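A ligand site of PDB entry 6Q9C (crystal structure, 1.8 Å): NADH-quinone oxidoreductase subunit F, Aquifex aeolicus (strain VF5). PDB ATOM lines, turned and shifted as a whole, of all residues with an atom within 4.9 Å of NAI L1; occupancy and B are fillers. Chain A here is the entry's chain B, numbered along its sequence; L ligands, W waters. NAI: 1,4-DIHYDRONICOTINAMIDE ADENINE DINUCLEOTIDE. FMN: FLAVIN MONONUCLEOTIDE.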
ATOM      1  N   GLY A  66     -11.179 -33.982  14.159  1.00  0.00           N
ATOM      2  CA  GLY A  66     -11.949 -32.798  14.579  1.00  0.00           C
ATOM      3  C   GLY A  66     -12.903 -32.341  13.486  1.00  0.00           C
ATOM      4  O   GLY A  66     -13.851 -31.602  13.823  1.00  0.00           O
ATOM      5  N   GLY A  67     -12.652 -32.736  12.229  1.00  0.00           N
ATOM      6  CA  GLY A  67     -13.580 -32.466  11.113  1.00  0.00           C
ATOM      7  C   GLY A  67     -12.894 -32.005   9.841  1.00  0.00           C
ATOM      8  O   GLY A  67     -13.501 -32.183   8.777  1.00  0.00           O
ATOM      9  N   ALA A  68     -11.675 -31.460   9.911  1.00  0.00           N
ATOM     10  CA  ALA A  68     -10.969 -30.898   8.729  1.00  0.00           C
ATOM     11  C   ALA A  68     -10.097 -31.964   8.058  1.00  0.00           C
ATOM     12  O   ALA A  68      -9.765 -31.774   6.869  1.00  0.00           O
ATOM     13  CB  ALA A  68     -10.150 -29.705   9.126  1.00  0.00           C
ATOM     14  N   PHE A  70      -6.904 -32.796   8.441  1.00  0.00           N
ATOM     15  CA  PHE A  70      -5.482 -32.472   8.201  1.00  0.00           C
ATOM     16  C   PHE A  70      -4.610 -33.652   8.638  1.00  0.00           C
ATOM     17  O   PHE A  70      -4.841 -34.226   9.702  1.00  0.00           O
ATOM     18  CB  PHE A  70      -5.051 -31.189   8.918  1.00  0.00           C
ATOM     19  CG  PHE A  70      -3.750 -30.641   8.427  1.00  0.00           C
ATOM     20  CD1 PHE A  70      -3.702 -29.768   7.345  1.00  0.00           C
ATOM     21  CD2 PHE A  70      -2.547 -31.017   9.014  1.00  0.00           C
ATOM     22  CE1 PHE A  70      -2.495 -29.276   6.889  1.00  0.00           C
ATOM     23  CE2 PHE A  70      -1.337 -30.518   8.546  1.00  0.00           C
ATOM     24  CZ  PHE A  70      -1.319 -29.642   7.484  1.00  0.00           C
ATOM     25  N   LYS A  75       1.262 -32.290  10.651  1.00  0.00           N
ATOM     26  CA  LYS A  75       1.025 -31.177  11.599  1.00  0.00           C
ATOM     27  C   LYS A  75       2.140 -31.183  12.654  1.00  0.00           C
ATOM     28  O   LYS A  75       2.703 -30.112  12.940  1.00  0.00           O
ATOM     29  CB  LYS A  75      -0.359 -31.266  12.265  1.00  0.00           C
ATOM     30  CG  LYS A  75      -0.745 -30.050  13.087  1.00  0.00           C
ATOM     31  CD  LYS A  75      -1.985 -30.246  13.933  1.00  0.00           C
ATOM     32  CE  LYS A  75      -3.249 -30.413  13.116  1.00  0.00           C
ATOM     33  NZ  LYS A  75      -4.466 -30.251  13.931  1.00  0.00           N
ATOM     34  N   PHE A  78       5.507 -29.946  11.200  1.00  0.00           N
ATOM     35  CA  PHE A  78       5.502 -28.454  11.108  1.00  0.00           C
ATOM     36  C   PHE A  78       5.880 -27.860  12.469  1.00  0.00           C
ATOM     37  O   PHE A  78       6.733 -26.956  12.497  1.00  0.00           O
ATOM     38  CB  PHE A  78       4.162 -27.917  10.608  1.00  0.00           C
ATOM     39  CG  PHE A  78       3.996 -27.926   9.111  1.00  0.00           C
ATOM     40  CD1 PHE A  78       4.811 -27.135   8.307  1.00  0.00           C
ATOM     41  CD2 PHE A  78       3.020 -28.700   8.513  1.00  0.00           C
ATOM     42  CE1 PHE A  78       4.666 -27.154   6.922  1.00  0.00           C
ATOM     43  CE2 PHE A  78       2.869 -28.707   7.134  1.00  0.00           C
ATOM     44  CZ  PHE A  78       3.687 -27.935   6.337  1.00  0.00           C
ATOM     45  N   GLU A  94     -15.919 -30.056  21.579  1.00  0.00           N
ATOM     46  CA  GLU A  94     -17.018 -30.720  20.832  1.00  0.00           C
ATOM     47  C   GLU A  94     -18.372 -30.023  21.017  1.00  0.00           C
ATOM     48  O   GLU A  94     -19.088 -30.357  21.971  1.00  0.00           O
ATOM     49  CB  GLU A  94     -17.149 -32.178  21.284  1.00  0.00           C
ATOM     50  CG  GLU A  94     -18.266 -32.930  20.601  1.00  0.00           C
ATOM     51  CD  GLU A  94     -18.179 -34.421  20.838  1.00  0.00           C
ATOM     52  OE1 GLU A  94     -18.404 -34.843  21.993  1.00  0.00           O
ATOM     53  OE2 GLU A  94     -17.849 -35.138  19.876  1.00  0.00           O
ATOM     54  N   SER A  95     -18.721 -29.085  20.136  1.00  0.00           N
ATOM     55  CA  SER A  95     -19.986 -28.307  20.209  1.00  0.00           C
ATOM     56  C   SER A  95     -20.707 -28.241  18.858  1.00  0.00           C
ATOM     57  O   SER A  95     -21.746 -27.556  18.815  1.00  0.00           O
ATOM     58  CB  SER A  95     -19.721 -26.936  20.766  1.00  0.00           C
ATOM     59  OG  SER A  95     -19.241 -27.013  22.102  1.00  0.00           O
ATOM     60  N   GLU A  96     -20.249 -28.944  17.821  1.00  0.00           N
ATOM     61  CA  GLU A  96     -20.974 -29.043  16.518  1.00  0.00           C
ATOM     62  C   GLU A  96     -22.322 -29.721  16.760  1.00  0.00           C
ATOM     63  O   GLU A  96     -22.382 -30.771  17.387  1.00  0.00           O
ATOM     64  CB  GLU A  96     -20.169 -29.839  15.492  1.00  0.00           C
ATOM     65  CG  GLU A  96     -20.772 -29.836  14.095  1.00  0.00           C
ATOM     66  CD  GLU A  96     -20.603 -28.541  13.327  1.00  0.00           C
ATOM     67  OE1 GLU A  96     -20.212 -27.514  13.948  1.00  0.00           O
ATOM     68  OE2 GLU A  96     -20.868 -28.552  12.104  1.00  0.00           O
ATOM     69  N   THR A  99     -22.995 -33.745  17.239  1.00  0.00           N
ATOM     70  CA  THR A  99     -21.636 -34.305  17.462  1.00  0.00           C
ATOM     71  C   THR A  99     -21.439 -34.638  18.951  1.00  0.00           C
ATOM     72  O   THR A  99     -21.420 -33.715  19.801  1.00  0.00           O
ATOM     73  CB  THR A  99     -20.554 -33.395  16.875  1.00  0.00           C
ATOM     74  OG1 THR A  99     -21.016 -32.998  15.585  1.00  0.00           O
ATOM     75  CG2 THR A  99     -19.216 -34.088  16.738  1.00  0.00           C
ATOM     76  N   ASP A 102     -16.713 -37.475  20.835  1.00  0.00           N
ATOM     77  CA  ASP A 102     -15.531 -37.250  21.725  1.00  0.00           C
ATOM     78  C   ASP A 102     -15.881 -37.546  23.195  1.00  0.00           C
ATOM     79  O   ASP A 102     -15.015 -38.076  23.915  1.00  0.00           O
ATOM     80  CB  ASP A 102     -14.988 -35.824  21.605  1.00  0.00           C
ATOM     81  CG  ASP A 102     -14.452 -35.487  20.231  1.00  0.00           C
ATOM     82  OD1 ASP A 102     -14.218 -36.415  19.440  1.00  0.00           O
ATOM     83  OD2 ASP A 102     -14.256 -34.287  19.961  1.00  0.00           O
ATOM     84  N   TYR A 179     -19.225 -21.863  21.301  1.00  0.00           N
ATOM     85  CA  TYR A 179     -18.886 -22.786  20.181  1.00  0.00           C
ATOM     86  C   TYR A 179     -17.571 -22.371  19.523  1.00  0.00           C
ATOM     87  O   TYR A 179     -16.795 -23.245  19.125  1.00  0.00           O
ATOM     88  CB  TYR A 179     -20.027 -22.779  19.171  1.00  0.00           C
ATOM     89  CG  TYR A 179     -19.778 -23.372  17.815  1.00  0.00           C
ATOM     90  CD1 TYR A 179     -19.783 -24.741  17.597  1.00  0.00           C
ATOM     91  CD2 TYR A 179     -19.655 -22.549  16.711  1.00  0.00           C
ATOM     92  CE1 TYR A 179     -19.633 -25.264  16.326  1.00  0.00           C
ATOM     93  CE2 TYR A 179     -19.504 -23.066  15.427  1.00  0.00           C
ATOM     94  CZ  TYR A 179     -19.497 -24.425  15.234  1.00  0.00           C
ATOM     95  OH  TYR A 179     -19.370 -24.908  13.964  1.00  0.00           O
ATOM     96  N   GLU A 184      -9.334 -23.536  16.880  1.00  0.00           N
ATOM     97  CA  GLU A 184      -8.048 -23.802  17.590  1.00  0.00           C
ATOM     98  C   GLU A 184      -7.412 -22.501  18.094  1.00  0.00           C
ATOM     99  O   GLU A 184      -6.832 -22.541  19.190  1.00  0.00           O
ATOM    100  CB  GLU A 184      -7.073 -24.594  16.710  1.00  0.00           C
ATOM    101  CG  GLU A 184      -6.729 -23.909  15.401  1.00  0.00           C
ATOM    102  CD  GLU A 184      -5.713 -24.634  14.540  1.00  0.00           C
ATOM    103  OE1 GLU A 184      -5.233 -25.716  14.968  1.00  0.00           O
ATOM    104  OE2 GLU A 184      -5.394 -24.110  13.447  1.00  0.00           O
ATOM    105  N   TYR A 204      -0.219 -20.521  11.612  1.00  0.00           N
ATOM    106  CA  TYR A 204      -0.908 -21.664  12.249  1.00  0.00           C
ATOM    107  C   TYR A 204      -0.303 -21.863  13.638  1.00  0.00           C
ATOM    108  O   TYR A 204       0.825 -21.454  13.903  1.00  0.00           O
ATOM    109  CB  TYR A 204      -0.833 -22.889  11.326  1.00  0.00           C
ATOM    110  CG  TYR A 204      -1.633 -22.683  10.069  1.00  0.00           C
ATOM    111  CD1 TYR A 204      -3.010 -22.884  10.067  1.00  0.00           C
ATOM    112  CD2 TYR A 204      -1.047 -22.194   8.916  1.00  0.00           C
ATOM    113  CE1 TYR A 204      -3.774 -22.647   8.938  1.00  0.00           C
ATOM    114  CE2 TYR A 204      -1.794 -21.960   7.772  1.00  0.00           C
ATOM    115  CZ  TYR A 204      -3.158 -22.187   7.783  1.00  0.00           C
ATOM    116  OH  TYR A 204      -3.899 -21.930   6.669  1.00  0.00           O
ATOM    117  N   PRO A 205      -1.078 -22.454  14.589  1.00  0.00           N
ATOM    118  CA  PRO A 205      -0.587 -22.648  15.953  1.00  0.00           C
ATOM    119  C   PRO A 205       0.779 -23.337  15.994  1.00  0.00           C
ATOM    120  O   PRO A 205       1.546 -23.032  16.895  1.00  0.00           O
ATOM    121  CB  PRO A 205      -1.680 -23.506  16.598  1.00  0.00           C
ATOM    122  CG  PRO A 205      -2.935 -23.169  15.835  1.00  0.00           C
ATOM    123  CD  PRO A 205      -2.461 -22.912  14.415  1.00  0.00           C
ATOM    124  N   VAL A 206       1.059 -24.233  15.033  1.00  0.00           N
ATOM    125  CA  VAL A 206       2.334 -25.017  14.999  1.00  0.00           C
ATOM    126  C   VAL A 206       3.527 -24.073  14.816  1.00  0.00           C
ATOM    127  O   VAL A 206       4.638 -24.472  15.170  1.00  0.00           O
ATOM    128  CB  VAL A 206       2.320 -26.121  13.915  1.00  0.00           C
ATOM    129  CG1 VAL A 206       1.378 -27.258  14.290  1.00  0.00           C
ATOM    130  CG2 VAL A 206       1.998 -25.574  12.535  1.00  0.00           C
ATOM    131  N   VAL A 217      -2.587 -28.355  18.193  1.00  0.00           N
ATOM    132  CA  VAL A 217      -3.994 -28.623  18.613  1.00  0.00           C
ATOM    133  C   VAL A 217      -4.458 -29.860  17.857  1.00  0.00           C
ATOM    134  O   VAL A 217      -4.425 -29.857  16.605  1.00  0.00           O
ATOM    135  CB  VAL A 217      -4.933 -27.426  18.368  1.00  0.00           C
ATOM    136  CG1 VAL A 217      -6.342 -27.724  18.885  1.00  0.00           C
ATOM    137  CG2 VAL A 217      -4.379 -26.152  18.980  1.00  0.00           C
ATOM    138  N   ASN A 219      -7.744 -32.974  18.039  1.00  0.00           N
ATOM    139  CA  ASN A 219      -9.077 -33.390  18.522  1.00  0.00           C
ATOM    140  C   ASN A 219      -8.912 -34.630  19.420  1.00  0.00           C
ATOM    141  O   ASN A 219      -7.993 -35.433  19.158  1.00  0.00           O
ATOM    142  CB  ASN A 219      -9.995 -33.630  17.329  1.00  0.00           C
ATOM    143  CG  ASN A 219     -11.309 -34.284  17.712  1.00  0.00           C
ATOM    144  OD1 ASN A 219     -11.455 -35.481  17.554  1.00  0.00           O
ATOM    145  ND2 ASN A 219     -12.232 -33.495  18.233  1.00  0.00           N
ATOM    146  N   LEU A 296     -22.559 -28.335   8.851  1.00  0.00           N
ATOM    147  CA  LEU A 296     -21.573 -28.074   7.759  1.00  0.00           C
ATOM    148  C   LEU A 296     -22.180 -28.355   6.379  1.00  0.00           C
ATOM    149  O   LEU A 296     -22.093 -27.468   5.498  1.00  0.00           O
ATOM    150  CB  LEU A 296     -20.344 -28.953   8.015  1.00  0.00           C
ATOM    151  CG  LEU A 296     -19.167 -28.788   7.052  1.00  0.00           C
ATOM    152  CD1 LEU A 296     -18.582 -27.383   7.123  1.00  0.00           C
ATOM    153  CD2 LEU A 296     -18.098 -29.832   7.337  1.00  0.00           C
ATOM    154  N   GLY A 317     -16.005 -34.205   7.133  1.00  0.00           N
ATOM    155  CA  GLY A 317     -16.406 -33.500   8.360  1.00  0.00           C
ATOM    156  C   GLY A 317     -16.106 -34.326   9.602  1.00  0.00           C
ATOM    157  O   GLY A 317     -15.098 -35.059   9.613  1.00  0.00           O
ATOM    158  N   THR A 318     -16.973 -34.236  10.602  1.00  0.00           N
ATOM    159  CA  THR A 318     -16.805 -34.904  11.922  1.00  0.00           C
ATOM    160  C   THR A 318     -17.273 -36.361  11.835  1.00  0.00           C
ATOM    161  O   THR A 318     -17.021 -37.105  12.788  1.00  0.00           O
ATOM    162  CB  THR A 318     -17.582 -34.151  12.995  1.00  0.00           C
ATOM    163  OG1 THR A 318     -18.929 -34.048  12.544  1.00  0.00           O
ATOM    164  CG2 THR A 318     -17.059 -32.757  13.268  1.00  0.00           C
ATOM    165  N   GLY A 393     -13.207 -20.453  10.152  1.00  0.00           N
ATOM    166  CA  GLY A 393     -14.105 -21.401   9.459  1.00  0.00           C
ATOM    167  C   GLY A 393     -15.587 -21.127   9.686  1.00  0.00           C
ATOM    168  O   GLY A 393     -16.372 -21.603   8.852  1.00  0.00           O
HETATM  169  PA  NAI L   1      -8.421 -26.126   8.602  1.00  0.00           P
HETATM  170  O1A NAI L   1      -8.592 -27.044   7.444  1.00  0.00           O
HETATM  171  O2A NAI L   1      -8.139 -24.671   8.257  1.00  0.00           O
HETATM  172  O5B NAI L   1      -7.217 -26.625   9.562  1.00  0.00           O
HETATM  173  C5B NAI L   1      -7.242 -27.964  10.088  1.00  0.00           C
HETATM  174  C4B NAI L   1      -6.025 -28.196  10.951  1.00  0.00           C
HETATM  175  O4B NAI L   1      -4.848 -28.264  10.114  1.00  0.00           O
HETATM  176  C3B NAI L   1      -5.742 -27.093  11.976  1.00  0.00           C
HETATM  177  O3B NAI L   1      -5.196 -27.642  13.167  1.00  0.00           O
HETATM  178  C2B NAI L   1      -4.751 -26.196  11.244  1.00  0.00           C
HETATM  179  O2B NAI L   1      -3.891 -25.496  12.130  1.00  0.00           O
HETATM  180  C1B NAI L   1      -3.945 -27.222  10.444  1.00  0.00           C
HETATM  181  N9A NAI L   1      -3.389 -26.682   9.208  1.00  0.00           N
HETATM  182  C8A NAI L   1      -4.079 -26.341   8.066  1.00  0.00           C
HETATM  183  N7A NAI L   1      -3.328 -25.801   7.133  1.00  0.00           N
HETATM  184  C5A NAI L   1      -2.061 -25.780   7.693  1.00  0.00           C
HETATM  185  C6A NAI L   1      -0.822 -25.309   7.223  1.00  0.00           C
HETATM  186  N6A NAI L   1      -0.660 -24.701   6.042  1.00  0.00           N
HETATM  187  N1A NAI L   1       0.257 -25.450   8.036  1.00  0.00           N
HETATM  188  C2A NAI L   1       0.080 -26.022   9.233  1.00  0.00           C
HETATM  189  N3A NAI L   1      -1.035 -26.487   9.785  1.00  0.00           N
HETATM  190  C4A NAI L   1      -2.084 -26.331   8.969  1.00  0.00           C
HETATM  191  O3  NAI L   1      -9.722 -26.168   9.512  1.00  0.00           O
HETATM  192  PN  NAI L   1     -10.296 -25.481  10.820  1.00  0.00           P
HETATM  193  O1N NAI L   1     -10.847 -24.122  10.414  1.00  0.00           O
HETATM  194  O2N NAI L   1      -9.335 -25.484  11.947  1.00  0.00           O
HETATM  195  O5D NAI L   1     -11.572 -26.424  11.160  1.00  0.00           O
HETATM  196  C5D NAI L   1     -12.750 -26.589  10.343  1.00  0.00           C
HETATM  197  C4D NAI L   1     -13.483 -27.837  10.769  1.00  0.00           C
HETATM  198  O4D NAI L   1     -13.911 -27.728  12.142  1.00  0.00           O
HETATM  199  C3D NAI L   1     -14.765 -28.145   9.987  1.00  0.00           C
HETATM  200  O3D NAI L   1     -14.483 -29.029   8.911  1.00  0.00           O
HETATM  201  C2D NAI L   1     -15.700 -28.780  11.033  1.00  0.00           C
HETATM  202  O2D NAI L   1     -15.995 -30.131  10.692  1.00  0.00           O
HETATM  203  C1D NAI L   1     -14.869 -28.742  12.329  1.00  0.00           C
HETATM  204  N1N NAI L   1     -15.642 -28.471  13.526  1.00  0.00           N
HETATM  205  C2N NAI L   1     -15.805 -29.447  14.548  1.00  0.00           C
HETATM  206  C3N NAI L   1     -16.519 -29.225  15.671  1.00  0.00           C
HETATM  207  C7N NAI L   1     -16.668 -30.314  16.643  1.00  0.00           C
HETATM  208  O7N NAI L   1     -17.547 -30.230  17.517  1.00  0.00           O
HETATM  209  N7N NAI L   1     -15.855 -31.363  16.547  1.00  0.00           N
HETATM  210  C4N NAI L   1     -17.186 -27.921  15.906  1.00  0.00           C
HETATM  211  C5N NAI L   1     -16.952 -26.969  14.785  1.00  0.00           C
HETATM  212  C6N NAI L   1     -16.243 -27.262  13.704  1.00  0.00           C
HETATM  213  N1  FMN L   2     -12.110 -29.039  16.541  1.00  0.00           N
HETATM  214  C2  FMN L   2     -12.320 -29.856  17.609  1.00  0.00           C
HETATM  215  O2  FMN L   2     -11.555 -30.792  17.873  1.00  0.00           O
HETATM  216  N3  FMN L   2     -13.382 -29.600  18.469  1.00  0.00           N
HETATM  217  C4  FMN L   2     -14.268 -28.534  18.374  1.00  0.00           C
HETATM  218  O4  FMN L   2     -15.196 -28.419  19.174  1.00  0.00           O
HETATM  219  C4A FMN L   2     -13.996 -27.642  17.253  1.00  0.00           C
HETATM  220  N5  FMN L   2     -14.747 -26.582  17.113  1.00  0.00           N
HETATM  221  C5A FMN L   2     -14.472 -25.732  16.051  1.00  0.00           C
HETATM  222  C6  FMN L   2     -15.269 -24.585  15.878  1.00  0.00           C
HETATM  223  C7  FMN L   2     -15.074 -23.733  14.794  1.00  0.00           C
HETATM  224  C7M FMN L   2     -15.983 -22.536  14.628  1.00  0.00           C
HETATM  225  C8  FMN L   2     -14.058 -24.020  13.868  1.00  0.00           C
HETATM  226  C8M FMN L   2     -13.851 -23.164  12.642  1.00  0.00           C
HETATM  227  C9  FMN L   2     -13.251 -25.132  14.046  1.00  0.00           C
HETATM  228  C9A FMN L   2     -13.450 -25.998  15.121  1.00  0.00           C
HETATM  229  N10 FMN L   2     -12.658 -27.159  15.319  1.00  0.00           N
HETATM  230  C10 FMN L   2     -12.903 -27.995  16.378  1.00  0.00           C
HETATM  231  C1' FMN L   2     -11.501 -27.452  14.464  1.00  0.00           C
HETATM  232  C2' FMN L   2     -10.203 -26.957  15.073  1.00  0.00           C
HETATM  233  O2' FMN L   2      -9.979 -25.582  14.739  1.00  0.00           O
HETATM  234  C3' FMN L   2      -9.008 -27.788  14.617  1.00  0.00           C
HETATM  235  O3' FMN L   2      -9.016 -27.958  13.200  1.00  0.00           O
HETATM  236  C4' FMN L   2      -8.897 -29.179  15.237  1.00  0.00           C
HETATM  237  O4' FMN L   2      -9.134 -29.128  16.637  1.00  0.00           O
HETATM  238  C5' FMN L   2      -7.526 -29.756  14.933  1.00  0.00           C
HETATM  239  O5' FMN L   2      -7.467 -31.118  15.422  1.00  0.00           O
HETATM  240  P   FMN L   2      -7.490 -32.333  14.390  1.00  0.00           P
HETATM  241  O1P FMN L   2      -8.862 -32.508  13.777  1.00  0.00           O
HETATM  242  O2P FMN L   2      -6.436 -32.056  13.343  1.00  0.00           O
HETATM  243  O3P FMN L   2      -7.057 -33.548  15.242  1.00  0.00           O
HETATM  244  O   HOH W   1     -16.029 -33.852  17.997  1.00  0.00           O
HETATM  245  O   HOH W   2      -7.360 -22.583   9.477  1.00  0.00           O
HETATM  246  O   HOH W   3     -10.815 -21.586  11.322  1.00  0.00           O
HETATM  247  O   HOH W   4      -4.959 -25.405   4.823  1.00  0.00           O
HETATM  248  O   HOH W   5     -17.388 -25.400  11.083  1.00  0.00           O
HETATM  249  O   HOH W   6       2.703 -24.303   7.289  1.00  0.00           O
HETATM  250  O   HOH W   7      -7.722 -23.232  12.022  1.00  0.00           O
HETATM  251  O   HOH W   8     -11.907 -23.652   7.921  1.00  0.00           O
HETATM  252  O   HOH W   9      -6.555 -27.882   5.662  1.00  0.00           O
HETATM  253  O   HOH W  10     -11.045 -27.685   6.032  1.00  0.00           O
HETATM  254  O   HOH W  11     -18.808 -30.166  11.136  1.00  0.00           O
HETATM  255  O   HOH W  12      -6.667 -23.811   6.062  1.00  0.00           O
HETATM  256  O   HOH W  13      -1.563 -26.113  13.030  1.00  0.00           O
HETATM  257  O   HOH W  14     -13.649 -27.701   6.823  1.00  0.00           O
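Merely in contact with NAI L1: Phe 70 (3.1 Å), Tyr 179 (3.3 Å), Glu 94 (3.4 Å), Tyr 204 (3.4 Å), Ala 68 (3.5 Å), Pro 205 (3.7 Å), Thr 318 (3.8 Å), Val 206 (3.8 Å) and Leu 296 (3.97 Å). Hydrophobic or aromatic side chains that line NAI L1: Ala 68, Phe 70, Tyr 179, Tyr 204, Pro 205, Val 206 and Leu 296. Within 4 Å of NAI L1: Gly 66, Gly 67, Ala 68, Phe 70, Lys 75, Glu 94, Ser 95, Glu 96, Tyr 179, Glu 184, Tyr 204, Pro 205, Val 206, Leu 296 and Thr 318. Along chain A the residues within 4 Å of NAI L1 span positions 66 to 318.
O3' of FMN L2 is in hydrogen-bond range of O2N of NAI L1 (2.8 Å).
The side-chain hydroxyl (OH) of Tyr 179 lies within hydrogen-bond range of the side-chain carboxylate (OE1) of Glu 96. OG1 of Thr 99 sits at hydrogen-bond distance from O of Glu 96 (3.2 Å). The side-chain amino group (NZ) of Lys 75 sits at hydrogen-bond distance from the backbone carbonyl oxygen (O) of Val 217, 2.7 Å away. The side-chain carboxylate (OE2) of Glu 94 is in hydrogen-bond range of the backbone NH (N) of Asp 102 (2.8 Å).
Water W3 bridges O1N of NAI L1 and N of Gly 393. Water W7 bridges O2N of NAI L1 and OE2 of Glu 184. Water W12 lies within hydrogen-bond range of an oxygen (O2A) of NAI L1 (2.8 Å) and the side-chain hydroxyl of Tyr 204 (3.4 Å). Water W11 bridges the side-chain carboxylate of Glu 96 (2.8 Å) and an oxygen (O2D) of NAI L1 (2.8 Å). Water W1 lies within hydrogen-bond range of OD2 of Asp 102 (2.7 Å), N7N of NAI L1 (2.9 Å) and OE2 of Glu 94 (2.9 Å).
ND2 of Asn 219 is in hydrogen-bond range of O2 of FMN L2. An oxygen (O2P) of FMN L2 is in salt-bridge range of the side-chain amino group of Lys 75, 2.7 Å away. A nitrogen (N7N) of NAI L1 lies close to the backbone carbonyl oxygen (O) of Gly 66 (3.4 Å). N of Glu 94 is in hydrogen-bond range of O4 of FMN L2 (3.0 Å). N of Gly 66 sits at hydrogen-bond distance from O1P of FMN L2 (2.8 Å). The side-chain amino group (NZ) of Lys 75 is in hydrogen-bond range of an oxygen (O3B) of NAI L1 (2.8 Å). The backbone NH of Glu 184 sits at hydrogen-bond distance from an oxygen (O2') of FMN L2 (3.0 Å). The backbone NH of Ser 95 lies within hydrogen-bond range of an oxygen (O7N) of NAI L1 (3.1 Å). OE2 of Glu 184 lies within hydrogen-bond range of O2B of NAI L1 (2.4 Å). The backbone NH of Asn 219 lies within hydrogen-bond range of an oxygen (O3P) of FMN L2 (2.9 Å). N of Glu 96 sits at hydrogen-bond distance from O7N of NAI L1, at 3.0 Å. O3D of NAI L1 is in hydrogen-bond range of O of Gly 67.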
